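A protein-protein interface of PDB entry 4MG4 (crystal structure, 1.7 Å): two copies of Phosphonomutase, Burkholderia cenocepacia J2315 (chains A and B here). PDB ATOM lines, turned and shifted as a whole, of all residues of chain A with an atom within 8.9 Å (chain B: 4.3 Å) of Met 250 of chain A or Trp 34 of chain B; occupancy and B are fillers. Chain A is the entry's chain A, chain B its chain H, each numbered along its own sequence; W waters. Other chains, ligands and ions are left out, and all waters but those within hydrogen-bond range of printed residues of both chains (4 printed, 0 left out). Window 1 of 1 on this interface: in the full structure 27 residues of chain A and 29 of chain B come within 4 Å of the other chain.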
ATOM      1  N   TRP A  34       7.834  21.992 -10.616  1.00  0.00           N
ATOM      2  CA  TRP A  34       8.528  23.249 -10.869  1.00  0.00           C
ATOM      3  C   TRP A  34       8.264  23.844 -12.255  1.00  0.00           C
ATOM      4  O   TRP A  34       8.779  24.915 -12.559  1.00  0.00           O
ATOM      5  CB  TRP A  34      10.037  23.070 -10.635  1.00  0.00           C
ATOM      6  CG  TRP A  34      10.596  22.020 -11.512  1.00  0.00           C
ATOM      7  CD1 TRP A  34      11.144  22.185 -12.764  1.00  0.00           C
ATOM      8  CD2 TRP A  34      10.693  20.636 -11.217  1.00  0.00           C
ATOM      9  NE1 TRP A  34      11.565  20.986 -13.263  1.00  0.00           N
ATOM     10  CE2 TRP A  34      11.322  20.012 -12.330  1.00  0.00           C
ATOM     11  CE3 TRP A  34      10.335  19.841 -10.131  1.00  0.00           C
ATOM     12  CZ2 TRP A  34      11.533  18.649 -12.377  1.00  0.00           C
ATOM     13  CZ3 TRP A  34      10.534  18.486 -10.200  1.00  0.00           C
ATOM     14  CH2 TRP A  34      11.182  17.911 -11.289  1.00  0.00           C
ATOM     15  N   ASP A  35       7.460  23.189 -13.081  1.00  0.00           N
ATOM     16  CA  ASP A  35       7.086  23.689 -14.403  1.00  0.00           C
ATOM     17  C   ASP A  35       5.956  22.836 -14.934  1.00  0.00           C
ATOM     18  O   ASP A  35       5.553  21.845 -14.299  1.00  0.00           O
ATOM     19  CB  ASP A  35       8.258  23.770 -15.414  1.00  0.00           C
ATOM     20  CG  ASP A  35       8.926  22.431 -15.692  1.00  0.00           C
ATOM     21  OD1 ASP A  35       8.401  21.332 -15.380  1.00  0.00           O
ATOM     22  OD2 ASP A  35      10.044  22.471 -16.289  1.00  0.00           O
ATOM     23  N   GLY A  37       5.751  20.830 -17.502  1.00  0.00           N
ATOM     24  CA  GLY A  37       6.107  19.462 -17.899  1.00  0.00           C
ATOM     25  C   GLY A  37       6.135  18.525 -16.701  1.00  0.00           C
ATOM     26  O   GLY A  37       5.623  17.390 -16.771  1.00  0.00           O
ATOM     27  N   SER A  38       6.776  18.977 -15.616  1.00  0.00           N
ATOM     28  CA  SER A  38       6.898  18.180 -14.398  1.00  0.00           C
ATOM     29  C   SER A  38       5.519  17.986 -13.740  1.00  0.00           C
ATOM     30  O   SER A  38       5.207  16.910 -13.192  1.00  0.00           O
ATOM     31  CB  SER A  38       7.942  18.750 -13.433  1.00  0.00           C
ATOM     32  OG  SER A  38       7.764  20.130 -13.090  1.00  0.00           O
ATOM     33  N   TRP A  55      12.280  26.004  -3.554  1.00  0.00           N
ATOM     34  CA  TRP A  55      13.684  25.691  -3.866  1.00  0.00           C
ATOM     35  C   TRP A  55      13.816  25.159  -5.297  1.00  0.00           C
ATOM     36  O   TRP A  55      14.675  25.637  -6.069  1.00  0.00           O
ATOM     37  CB  TRP A  55      14.232  24.640  -2.879  1.00  0.00           C
ATOM     38  CG  TRP A  55      15.713  24.549  -2.898  1.00  0.00           C
ATOM     39  CD1 TRP A  55      16.584  25.214  -2.078  1.00  0.00           C
ATOM     40  CD2 TRP A  55      16.520  23.788  -3.808  1.00  0.00           C
ATOM     41  NE1 TRP A  55      17.890  24.901  -2.414  1.00  0.00           N
ATOM     42  CE2 TRP A  55      17.874  24.025  -3.469  1.00  0.00           C
ATOM     43  CE3 TRP A  55      16.232  22.930  -4.855  1.00  0.00           C
ATOM     44  CZ2 TRP A  55      18.920  23.413  -4.137  1.00  0.00           C
ATOM     45  CZ3 TRP A  55      17.272  22.327  -5.522  1.00  0.00           C
ATOM     46  CH2 TRP A  55      18.596  22.575  -5.164  1.00  0.00           C
ATOM     47  N   SER A  56      12.980  24.179  -5.623  1.00  0.00           N
ATOM     48  CA  SER A  56      12.899  23.579  -6.966  1.00  0.00           C
ATOM     49  C   SER A  56      12.604  24.583  -8.079  1.00  0.00           C
ATOM     50  O   SER A  56      13.239  24.569  -9.151  1.00  0.00           O
ATOM     51  CB  SER A  56      11.795  22.475  -6.985  1.00  0.00           C
ATOM     52  OG  SER A  56      12.141  21.377  -6.159  1.00  0.00           O
ATOM     53  N   ALA A  59      15.692  26.873  -8.442  1.00  0.00           N
ATOM     54  CA  ALA A  59      16.778  26.146  -9.103  1.00  0.00           C
ATOM     55  C   ALA A  59      16.548  25.975 -10.607  1.00  0.00           C
ATOM     56  O   ALA A  59      17.417  26.279 -11.425  1.00  0.00           O
ATOM     57  CB  ALA A  59      16.971  24.803  -8.442  1.00  0.00           C
ATOM     58  N   ALA A  60      15.336  25.563 -10.960  1.00  0.00           N
ATOM     59  CA  ALA A  60      14.952  25.364 -12.363  1.00  0.00           C
ATOM     60  C   ALA A  60      15.115  26.649 -13.192  1.00  0.00           C
ATOM     61  O   ALA A  60      15.528  26.620 -14.366  1.00  0.00           O
ATOM     62  CB  ALA A  60      13.533  24.831 -12.440  1.00  0.00           C
ATOM     63  N   ASN A  61      14.892  27.785 -12.543  1.00  0.00           N
ATOM     64  CA  ASN A  61      14.913  29.098 -13.173  1.00  0.00           C
ATOM     65  C   ASN A  61      16.248  29.843 -12.964  1.00  0.00           C
ATOM     66  O   ASN A  61      16.358  30.996 -13.355  1.00  0.00           O
ATOM     67  CB  ASN A  61      13.719  29.949 -12.725  1.00  0.00           C
ATOM     68  CG  ASN A  61      12.424  29.492 -13.381  1.00  0.00           C
ATOM     69  OD1 ASN A  61      12.075  29.930 -14.480  1.00  0.00           O
ATOM     70  ND2 ASN A  61      11.769  28.555 -12.764  1.00  0.00           N
ATOM     71  N   PRO A 243      12.805  19.385  -2.070  1.00  0.00           N
ATOM     72  CA  PRO A 243      13.271  19.339  -3.482  1.00  0.00           C
ATOM     73  C   PRO A 243      13.741  17.971  -3.937  1.00  0.00           C
ATOM     74  O   PRO A 243      14.347  17.857  -5.013  1.00  0.00           O
ATOM     75  CB  PRO A 243      14.443  20.306  -3.476  1.00  0.00           C
ATOM     76  CG  PRO A 243      14.991  20.203  -2.122  1.00  0.00           C
ATOM     77  CD  PRO A 243      13.811  19.964  -1.174  1.00  0.00           C
ATOM     78  N   TYR A 244      13.470  16.906  -3.191  1.00  0.00           N
ATOM     79  CA  TYR A 244      13.860  15.552  -3.608  1.00  0.00           C
ATOM     80  C   TYR A 244      13.476  15.134  -5.043  1.00  0.00           C
ATOM     81  O   TYR A 244      14.356  14.629  -5.774  1.00  0.00           O
ATOM     82  CB  TYR A 244      13.299  14.554  -2.594  1.00  0.00           C
ATOM     83  CG  TYR A 244      13.570  13.100  -2.924  1.00  0.00           C
ATOM     84  CD1 TYR A 244      14.791  12.545  -2.630  1.00  0.00           C
ATOM     85  CD2 TYR A 244      12.585  12.293  -3.433  1.00  0.00           C
ATOM     86  CE1 TYR A 244      15.061  11.216  -2.896  1.00  0.00           C
ATOM     87  CE2 TYR A 244      12.840  10.951  -3.698  1.00  0.00           C
ATOM     88  CZ  TYR A 244      14.075  10.427  -3.420  1.00  0.00           C
ATOM     89  OH  TYR A 244      14.317   9.081  -3.651  1.00  0.00           O
ATOM     90  N   PRO A 245      12.217  15.381  -5.493  1.00  0.00           N
ATOM     91  CA  PRO A 245      11.878  15.002  -6.837  1.00  0.00           C
ATOM     92  C   PRO A 245      12.790  15.684  -7.890  1.00  0.00           C
ATOM     93  O   PRO A 245      13.339  15.015  -8.799  1.00  0.00           O
ATOM     94  CB  PRO A 245      10.418  15.430  -6.979  1.00  0.00           C
ATOM     95  CG  PRO A 245       9.875  15.366  -5.571  1.00  0.00           C
ATOM     96  CD  PRO A 245      11.014  15.831  -4.728  1.00  0.00           C
ATOM     97  N   TYR A 246      12.930  17.000  -7.752  1.00  0.00           N
ATOM     98  CA  TYR A 246      13.772  17.752  -8.693  1.00  0.00           C
ATOM     99  C   TYR A 246      15.206  17.235  -8.701  1.00  0.00           C
ATOM    100  O   TYR A 246      15.800  17.022  -9.802  1.00  0.00           O
ATOM    101  CB  TYR A 246      13.754  19.225  -8.316  1.00  0.00           C
ATOM    102  CG  TYR A 246      14.643  20.103  -9.177  1.00  0.00           C
ATOM    103  CD1 TYR A 246      14.220  20.562 -10.421  1.00  0.00           C
ATOM    104  CD2 TYR A 246      15.906  20.479  -8.728  1.00  0.00           C
ATOM    105  CE1 TYR A 246      15.044  21.356 -11.213  1.00  0.00           C
ATOM    106  CE2 TYR A 246      16.735  21.245  -9.523  1.00  0.00           C
ATOM    107  CZ  TYR A 246      16.283  21.705 -10.761  1.00  0.00           C
ATOM    108  OH  TYR A 246      17.113  22.531 -11.545  1.00  0.00           O
ATOM    109  N   LEU A 247      15.751  17.022  -7.501  1.00  0.00           N
ATOM    110  CA  LEU A 247      17.116  16.513  -7.340  1.00  0.00           C
ATOM    111  C   LEU A 247      17.324  15.138  -7.893  1.00  0.00           C
ATOM    112  O   LEU A 247      18.407  14.878  -8.493  1.00  0.00           O
ATOM    113  CB  LEU A 247      17.567  16.585  -5.886  1.00  0.00           C
ATOM    114  CG  LEU A 247      17.648  18.012  -5.348  1.00  0.00           C
ATOM    115  CD1 LEU A 247      17.969  17.992  -3.866  1.00  0.00           C
ATOM    116  CD2 LEU A 247      18.662  18.856  -6.121  1.00  0.00           C
ATOM    117  N   GLN A 248      16.335  14.260  -7.769  1.00  0.00           N
ATOM    118  CA  GLN A 248      16.442  12.943  -8.419  1.00  0.00           C
ATOM    119  C   GLN A 248      16.439  13.043  -9.947  1.00  0.00           C
ATOM    120  O   GLN A 248      17.238  12.350 -10.642  1.00  0.00           O
ATOM    121  CB  GLN A 248      15.315  12.022  -7.943  1.00  0.00           C
ATOM    122  CG  GLN A 248      15.473  11.689  -6.466  1.00  0.00           C
ATOM    123  CD  GLN A 248      16.742  10.914  -6.212  1.00  0.00           C
ATOM    124  OE1 GLN A 248      17.649  11.382  -5.525  1.00  0.00           O
ATOM    125  NE2 GLN A 248      16.839   9.751  -6.819  1.00  0.00           N
ATOM    126  N   ALA A 249      15.530  13.841 -10.488  1.00  0.00           N
ATOM    127  CA  ALA A 249      15.465  14.084 -11.951  1.00  0.00           C
ATOM    128  C   ALA A 249      16.827  14.619 -12.456  1.00  0.00           C
ATOM    129  O   ALA A 249      17.335  14.170 -13.515  1.00  0.00           O
ATOM    130  CB  ALA A 249      14.338  15.044 -12.290  1.00  0.00           C
ATOM    131  N   MET A 250      17.443  15.509 -11.698  1.00  0.00           N
ATOM    132  CA  MET A 250      18.677  16.115 -12.104  1.00  0.00           C
ATOM    133  C   MET A 250      19.844  15.127 -11.929  1.00  0.00           C
ATOM    134  O   MET A 250      20.839  15.221 -12.661  1.00  0.00           O
ATOM    135  CB  MET A 250      18.969  17.417 -11.342  1.00  0.00           C
ATOM    136  CG  MET A 250      18.020  18.581 -11.619  1.00  0.00           C
ATOM    137  SD  MET A 250      18.045  18.973 -13.392  1.00  0.00           S
ATOM    138  CE  MET A 250      16.564  18.251 -14.020  1.00  0.00           C
ATOM    139  N   LYS A 251      19.764  14.212 -10.960  1.00  0.00           N
ATOM    140  CA  LYS A 251      20.791  13.165 -10.837  1.00  0.00           C
ATOM    141  C   LYS A 251      20.842  12.301 -12.089  1.00  0.00           C
ATOM    142  O   LYS A 251      21.961  11.986 -12.637  1.00  0.00           O
ATOM    143  CB  LYS A 251      20.603  12.332  -9.556  1.00  0.00           C
ATOM    144  CG  LYS A 251      21.370  12.941  -8.373  1.00  0.00           C
ATOM    145  CD  LYS A 251      20.914  12.516  -6.970  1.00  0.00           C
ATOM    146  CE  LYS A 251      20.767  11.027  -6.822  1.00  0.00           C
ATOM    147  NZ  LYS A 251      20.300  10.729  -5.420  1.00  0.00           N
ATOM    148  N   THR A 252      19.669  11.956 -12.596  1.00  0.00           N
ATOM    149  CA  THR A 252      19.553  11.151 -13.793  1.00  0.00           C
ATOM    150  C   THR A 252      20.187  11.872 -14.990  1.00  0.00           C
ATOM    151  O   THR A 252      20.906  11.247 -15.798  1.00  0.00           O
ATOM    152  CB  THR A 252      18.093  10.832 -14.081  1.00  0.00           C
ATOM    153  OG1 THR A 252      17.637   9.888 -13.102  1.00  0.00           O
ATOM    154  CG2 THR A 252      17.929  10.242 -15.451  1.00  0.00           C
ATOM    155  N   LEU A 253      19.918  13.178 -15.074  1.00  0.00           N
ATOM    156  CA  LEU A 253      20.498  14.023 -16.107  1.00  0.00           C
ATOM    157  C   LEU A 253      22.032  14.062 -15.986  1.00  0.00           C
ATOM    158  O   LEU A 253      22.737  13.787 -16.988  1.00  0.00           O
ATOM    159  CB  LEU A 253      19.904  15.436 -16.086  1.00  0.00           C
ATOM    160  CG  LEU A 253      20.501  16.427 -17.100  1.00  0.00           C
ATOM    161  CD1 LEU A 253      20.303  15.972 -18.541  1.00  0.00           C
ATOM    162  CD2 LEU A 253      19.856  17.782 -16.870  1.00  0.00           C
ATOM    163  N   ALA A 254      22.550  14.388 -14.810  1.00  0.00           N
ATOM    164  CA  ALA A 254      24.011  14.437 -14.633  1.00  0.00           C
ATOM    165  C   ALA A 254      24.681  13.088 -14.955  1.00  0.00           C
ATOM    166  O   ALA A 254      25.779  13.043 -15.551  1.00  0.00           O
ATOM    167  CB  ALA A 254      24.363  14.876 -13.239  1.00  0.00           C
ATOM    168  N   ALA A 255      24.039  11.985 -14.589  1.00  0.00           N
ATOM    169  CA  ALA A 255      24.638  10.669 -14.851  1.00  0.00           C
ATOM    170  C   ALA A 255      24.681  10.344 -16.361  1.00  0.00           C
ATOM    171  O   ALA A 255      25.681   9.773 -16.853  1.00  0.00           O
ATOM    172  CB  ALA A 255      23.894   9.590 -14.096  1.00  0.00           C
ATOM    173  N   LEU A 256      23.618  10.690 -17.104  1.00  0.00           N
ATOM    174  CA  LEU A 256      23.663  10.588 -18.570  1.00  0.00           C
ATOM    175  C   LEU A 256      24.865  11.308 -19.176  1.00  0.00           C
ATOM    176  O   LEU A 256      25.521  10.755 -20.078  1.00  0.00           O
ATOM    177  CB  LEU A 256      22.409  11.143 -19.216  1.00  0.00           C
ATOM    178  CG  LEU A 256      21.189  10.262 -19.297  1.00  0.00           C
ATOM    179  CD1 LEU A 256      20.011  11.081 -19.807  1.00  0.00           C
ATOM    180  CD2 LEU A 256      21.428   9.057 -20.192  1.00  0.00           C
ATOM    181  N   VAL A 257      25.166  12.504 -18.674  1.00  0.00           N
ATOM    182  CA  VAL A 257      26.260  13.342 -19.193  1.00  0.00           C
ATOM    183  C   VAL A 257      27.614  12.675 -18.930  1.00  0.00           C
ATOM    184  O   VAL A 257      28.509  12.677 -19.798  1.00  0.00           O
ATOM    185  CB  VAL A 257      26.261  14.760 -18.579  1.00  0.00           C
ATOM    186  CG1 VAL A 257      27.455  15.586 -19.077  1.00  0.00           C
ATOM    187  CG2 VAL A 257      24.969  15.489 -18.910  1.00  0.00           C
ATOM    188  N   LYS A 258      27.778  12.163 -17.714  1.00  0.00           N
ATOM    189  CA  LYS A 258      29.025  11.518 -17.326  1.00  0.00           C
ATOM    190  C   LYS A 258      29.221  10.152 -17.942  1.00  0.00           C
ATOM    191  O   LYS A 258      30.356   9.770 -18.223  1.00  0.00           O
ATOM    192  CB  LYS A 258      29.116  11.434 -15.816  1.00  0.00           C
ATOM    193  CG  LYS A 258      29.418  12.787 -15.216  1.00  0.00           C
ATOM    194  CD  LYS A 258      29.607  12.658 -13.729  1.00  0.00           C
ATOM    195  CE  LYS A 258      28.813  13.735 -13.029  1.00  0.00           C
ATOM    196  NZ  LYS A 258      28.901  13.574 -11.560  1.00  0.00           N
ATOM    197  N   ASN B  32      20.710  18.209 -24.815  1.00  0.00           N
ATOM    198  CA  ASN B  32      19.759  19.289 -24.965  1.00  0.00           C
ATOM    199  C   ASN B  32      19.233  19.589 -23.565  1.00  0.00           C
ATOM    200  O   ASN B  32      18.682  18.714 -22.929  1.00  0.00           O
ATOM    201  CB  ASN B  32      18.623  18.952 -25.886  1.00  0.00           C
ATOM    202  CG  ASN B  32      19.020  18.957 -27.323  1.00  0.00           C
ATOM    203  OD1 ASN B  32      20.179  19.248 -27.653  1.00  0.00           O
ATOM    204  ND2 ASN B  32      18.105  18.599 -28.171  1.00  0.00           N
ATOM    205  N   VAL B  33      19.429  20.821 -23.140  1.00  0.00           N
ATOM    206  CA  VAL B  33      18.865  21.358 -21.903  1.00  0.00           C
ATOM    207  C   VAL B  33      17.676  22.262 -22.182  1.00  0.00           C
ATOM    208  O   VAL B  33      17.438  22.676 -23.307  1.00  0.00           O
ATOM    209  CB  VAL B  33      19.904  22.113 -21.087  1.00  0.00           C
ATOM    210  CG1 VAL B  33      21.006  21.179 -20.590  1.00  0.00           C
ATOM    211  CG2 VAL B  33      20.463  23.356 -21.781  1.00  0.00           C
ATOM    212  N   TRP B  34      16.900  22.578 -21.142  1.00  0.00           N
ATOM    213  CA  TRP B  34      15.587  23.160 -21.365  1.00  0.00           C
ATOM    214  C   TRP B  34      15.235  24.245 -20.362  1.00  0.00           C
ATOM    215  O   TRP B  34      14.155  24.871 -20.450  1.00  0.00           O
ATOM    216  CB  TRP B  34      14.505  22.101 -21.328  1.00  0.00           C
ATOM    217  CG  TRP B  34      14.509  21.304 -20.037  1.00  0.00           C
ATOM    218  CD1 TRP B  34      13.769  21.572 -18.909  1.00  0.00           C
ATOM    219  CD2 TRP B  34      15.269  20.118 -19.735  1.00  0.00           C
ATOM    220  NE1 TRP B  34      14.039  20.655 -17.933  1.00  0.00           N
ATOM    221  CE2 TRP B  34      14.966  19.750 -18.420  1.00  0.00           C
ATOM    222  CE3 TRP B  34      16.192  19.343 -20.454  1.00  0.00           C
ATOM    223  CZ2 TRP B  34      15.517  18.634 -17.819  1.00  0.00           C
ATOM    224  CZ3 TRP B  34      16.752  18.235 -19.852  1.00  0.00           C
ATOM    225  CH2 TRP B  34      16.394  17.872 -18.533  1.00  0.00           C
ATOM    226  N   ASP B  35      16.121  24.438 -19.408  1.00  0.00           N
ATOM    227  CA  ASP B  35      15.999  25.539 -18.472  1.00  0.00           C
ATOM    228  C   ASP B  35      17.352  25.807 -17.822  1.00  0.00           C
ATOM    229  O   ASP B  35      18.337  25.103 -18.081  1.00  0.00           O
ATOM    230  CB  ASP B  35      14.844  25.312 -17.442  1.00  0.00           C
ATOM    231  CG  ASP B  35      15.011  24.067 -16.564  1.00  0.00           C
ATOM    232  OD1 ASP B  35      16.102  23.453 -16.527  1.00  0.00           O
ATOM    233  OD2 ASP B  35      13.990  23.670 -15.830  1.00  0.00           O
ATOM    234  N   SER B  38      18.700  22.801 -15.572  1.00  0.00           N
ATOM    235  CA  SER B  38      19.266  21.689 -16.409  1.00  0.00           C
ATOM    236  C   SER B  38      20.587  22.100 -17.023  1.00  0.00           C
ATOM    237  O   SER B  38      21.545  21.289 -17.095  1.00  0.00           O
ATOM    238  CB  SER B  38      18.259  21.157 -17.445  1.00  0.00           C
ATOM    239  OG  SER B  38      17.673  22.131 -18.262  1.00  0.00           O
ATOM    240  N   VAL B  41      23.188  21.783 -14.351  1.00  0.00           N
ATOM    241  CA  VAL B  41      23.455  20.390 -14.027  1.00  0.00           C
ATOM    242  C   VAL B  41      24.387  19.796 -15.074  1.00  0.00           C
ATOM    243  O   VAL B  41      25.406  19.176 -14.752  1.00  0.00           O
ATOM    244  CB  VAL B  41      22.170  19.579 -13.905  1.00  0.00           C
ATOM    245  CG1 VAL B  41      22.416  18.067 -13.890  1.00  0.00           C
ATOM    246  CG2 VAL B  41      21.464  19.973 -12.598  1.00  0.00           C
ATOM    247  N   SER B  56      12.149  19.670 -25.983  1.00  0.00           N
ATOM    248  CA  SER B  56      12.330  19.670 -24.526  1.00  0.00           C
ATOM    249  C   SER B  56      11.848  20.979 -23.920  1.00  0.00           C
ATOM    250  O   SER B  56      11.178  20.974 -22.874  1.00  0.00           O
ATOM    251  CB  SER B  56      13.819  19.434 -24.134  1.00  0.00           C
ATOM    252  OG  SER B  56      14.259  18.147 -24.514  1.00  0.00           O
ATOM    253  N   VAL B  57      12.196  22.113 -24.529  1.00  0.00           N
ATOM    254  CA  VAL B  57      11.744  23.397 -24.021  1.00  0.00           C
ATOM    255  C   VAL B  57      10.226  23.516 -24.085  1.00  0.00           C
ATOM    256  O   VAL B  57       9.576  24.016 -23.135  1.00  0.00           O
ATOM    257  CB  VAL B  57      12.450  24.555 -24.787  1.00  0.00           C
ATOM    258  CG1 VAL B  57      11.823  25.874 -24.422  1.00  0.00           C
ATOM    259  CG2 VAL B  57      13.943  24.584 -24.471  1.00  0.00           C
ATOM    260  N   ALA B  60       8.684  21.128 -21.380  1.00  0.00           N
ATOM    261  CA  ALA B  60       8.856  21.598 -20.020  1.00  0.00           C
ATOM    262  C   ALA B  60       7.875  22.725 -19.742  1.00  0.00           C
ATOM    263  O   ALA B  60       7.416  22.868 -18.612  1.00  0.00           O
ATOM    264  CB  ALA B  60      10.244  22.062 -19.776  1.00  0.00           C
ATOM    265  N   VAL B  77      13.441  31.903 -22.499  1.00  0.00           N
ATOM    266  CA  VAL B  77      14.052  30.692 -21.961  1.00  0.00           C
ATOM    267  C   VAL B  77      15.514  30.707 -22.318  1.00  0.00           C
ATOM    268  O   VAL B  77      16.355  30.448 -21.481  1.00  0.00           O
ATOM    269  CB  VAL B  77      13.448  29.402 -22.564  1.00  0.00           C
ATOM    270  CG1 VAL B  77      14.232  28.178 -22.105  1.00  0.00           C
ATOM    271  CG2 VAL B  77      11.983  29.235 -22.171  1.00  0.00           C
ATOM    272  N   ILE B  81      18.941  30.424 -19.951  1.00  0.00           N
ATOM    273  CA  ILE B  81      19.906  29.328 -20.080  1.00  0.00           C
ATOM    274  C   ILE B  81      21.302  29.865 -20.340  1.00  0.00           C
ATOM    275  O   ILE B  81      22.284  29.387 -19.766  1.00  0.00           O
ATOM    276  CB  ILE B  81      19.450  28.366 -21.215  1.00  0.00           C
ATOM    277  CG1 ILE B  81      18.256  27.532 -20.768  1.00  0.00           C
ATOM    278  CG2 ILE B  81      20.592  27.461 -21.698  1.00  0.00           C
ATOM    279  CD1 ILE B  81      17.478  26.866 -21.901  1.00  0.00           C
ATOM    280  N   PRO B 245      17.520  13.301 -23.012  1.00  0.00           N
ATOM    281  CA  PRO B 245      17.893  13.642 -21.637  1.00  0.00           C
ATOM    282  C   PRO B 245      16.671  14.080 -20.787  1.00  0.00           C
ATOM    283  O   PRO B 245      16.516  13.620 -19.661  1.00  0.00           O
ATOM    284  CB  PRO B 245      18.882  14.799 -21.801  1.00  0.00           C
ATOM    285  CG  PRO B 245      19.480  14.549 -23.157  1.00  0.00           C
ATOM    286  CD  PRO B 245      18.352  14.044 -23.987  1.00  0.00           C
ATOM    287  N   TYR B 246      15.834  14.926 -21.371  1.00  0.00           N
ATOM    288  CA  TYR B 246      14.591  15.402 -20.701  1.00  0.00           C
ATOM    289  C   TYR B 246      13.699  14.225 -20.392  1.00  0.00           C
ATOM    290  O   TYR B 246      13.131  14.128 -19.263  1.00  0.00           O
ATOM    291  CB  TYR B 246      13.859  16.397 -21.637  1.00  0.00           C
ATOM    292  CG  TYR B 246      12.506  16.853 -21.125  1.00  0.00           C
ATOM    293  CD1 TYR B 246      12.436  17.818 -20.143  1.00  0.00           C
ATOM    294  CD2 TYR B 246      11.326  16.301 -21.588  1.00  0.00           C
ATOM    295  CE1 TYR B 246      11.215  18.238 -19.642  1.00  0.00           C
ATOM    296  CE2 TYR B 246      10.096  16.680 -21.043  1.00  0.00           C
ATOM    297  CZ  TYR B 246      10.062  17.655 -20.101  1.00  0.00           C
ATOM    298  OH  TYR B 246       8.821  18.063 -19.574  1.00  0.00           O
HETATM  299  O   HOH W   1       6.744  16.664 -19.609  1.00  0.00           O
HETATM  300  O   HOH W   2      11.790  25.077 -15.840  1.00  0.00           O
HETATM  301  O   HOH W   3      12.453  21.286 -15.771  1.00  0.00           O
HETATM  302  O   HOH W   4       9.976  19.213 -16.601  1.00  0.00           O
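Water W1 lies within hydrogen-bond range of OH of Tyr 246 of chain B and O of Gly 37 of chain A. Water W2 lies within hydrogen-bond range of OD2 of Asp 35 of chain B (2.6 Å) and OD2 of Asp 35 of chain A (3.2 Å). Water W3 lies within hydrogen-bond range of the indole nitrogen (NE1) of Trp 34 of chain A, the side-chain carboxylate (OD2) of Asp 35 of chain A, the indole nitrogen (NE1) of Trp 34 of chain B and the side-chain carboxylate (OD2) of Asp 35 of chain B. Water W4 lies within hydrogen-bond range of OD1 of Asp 35 of chain A (2.9 Å), N of Ser 38 of chain A (3.4 Å) and OH of Tyr 246 of chain B (3.4 Å).
OD1 of Asp 35 of chain A lies close to N of Gly 37 of chain A (3.4 Å). The side-chain hydroxyl (OG) of Ser 38 of chain A is in hydrogen-bond range of the side-chain carboxylate (OD1) of Asp 35 of chain A (2.7 Å). The side-chain hydroxyl (OG) of Ser 38 of chain B is in hydrogen-bond range of the backbone NH (N) of Trp 34 of chain B (3.0 Å). The side-chain carboxylate (OD1) of Asp 35 of chain B is in hydrogen-bond range of the side-chain hydroxyl (OG) of Ser 38 of chain B (2.7 Å).
Hydrophobic or aromatic side chains of chain A within 4 Å of the printed part of chain B: Ala 60, Met 250, Leu 253, Ala 254 and Leu 256. Hydrophobic or aromatic side chains of chain B within 4 Å of the printed part of chain A: Trp 34, Val 41, Ala 60, Pro 245 and Tyr 246.
Asp 35 of chain A touches Ala 60 of chain B, and with the chains exchanged Ala 60 of chain A touches Asp 35 of chain B. Positions printed for both chains: 34, 35, 38, 56, 60, 245 and 246. Of the 12 pairs that touch across the chains among the printed residues, 2 have their exchanged pair printed and touching as well.
Among the printed residues, pairs that only touch across the chains: Asp 35 of chain A with Ala 60 of chain B (3.3 Å), Gly 37 of chain A with Tyr 246 of chain B (3.5 Å), Ala 60 of chain A with Asp 35 of chain B (3.4 Å), Met 250 of chain A with Trp 34 of chain B (3.96 Å), Met 250 of chain A with Val 41 of chain B (3.5 Å), Leu 253 of chain A with Trp 34 of chain B (3.8 Å), Leu 253 of chain A with Ser 38 of chain B (3.8 Å), Leu 253 of chain A with Val 41 of chain B (3.9 Å), Leu 253 of chain A with Pro 245 of chain B (3.7 Å), Ala 254 of chain A with Val 41 of chain B (3.8 Å) and Leu 256 of chain A with Pro 245 of chain B (3.8 Å).
Printed residues of chain B within 4 Å of Gly 37 of chain A: Ala 60 and Tyr 246. Met 250 of chain A touches just these residues of chain B: Trp 34 (3.96 Å) and Val 41 (3.5 Å). Printed residues of chain B within 4 Å of Leu 253 of chain A: Trp 34, Ser 38, Val 41 and Pro 245. Of the printed residues of chain B, Leu 256 of chain A touches Pro 245 (3.8 Å). No residue of chain A comes within 4 Å of Val 33 of chain B. Of the printed residues of chain A, Ala 60 of chain B touches Asp 35 (3.3 Å) and Gly 37 (2.9 Å). Printed residues of chain A within 4 Å of Tyr 246 of chain B: Gly 37 (3.5 Å). The nearest residue of chain B that does not touch Met 250 of chain A is Ser 38 of chain B (4.2 Å). The nearest residue of chain A that does not touch Trp 34 of chain B is Asp 35 of chain A (4.6 Å). The nearest printed residue of chain B that does not touch Gly 37 of chain A is Ser 56 of chain B (7.3 Å).
The backbone NH of Gly 37 of chain A is in hydrogen-bond range of the backbone carbonyl oxygen of Ala 60 of chain B (2.9 Å).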
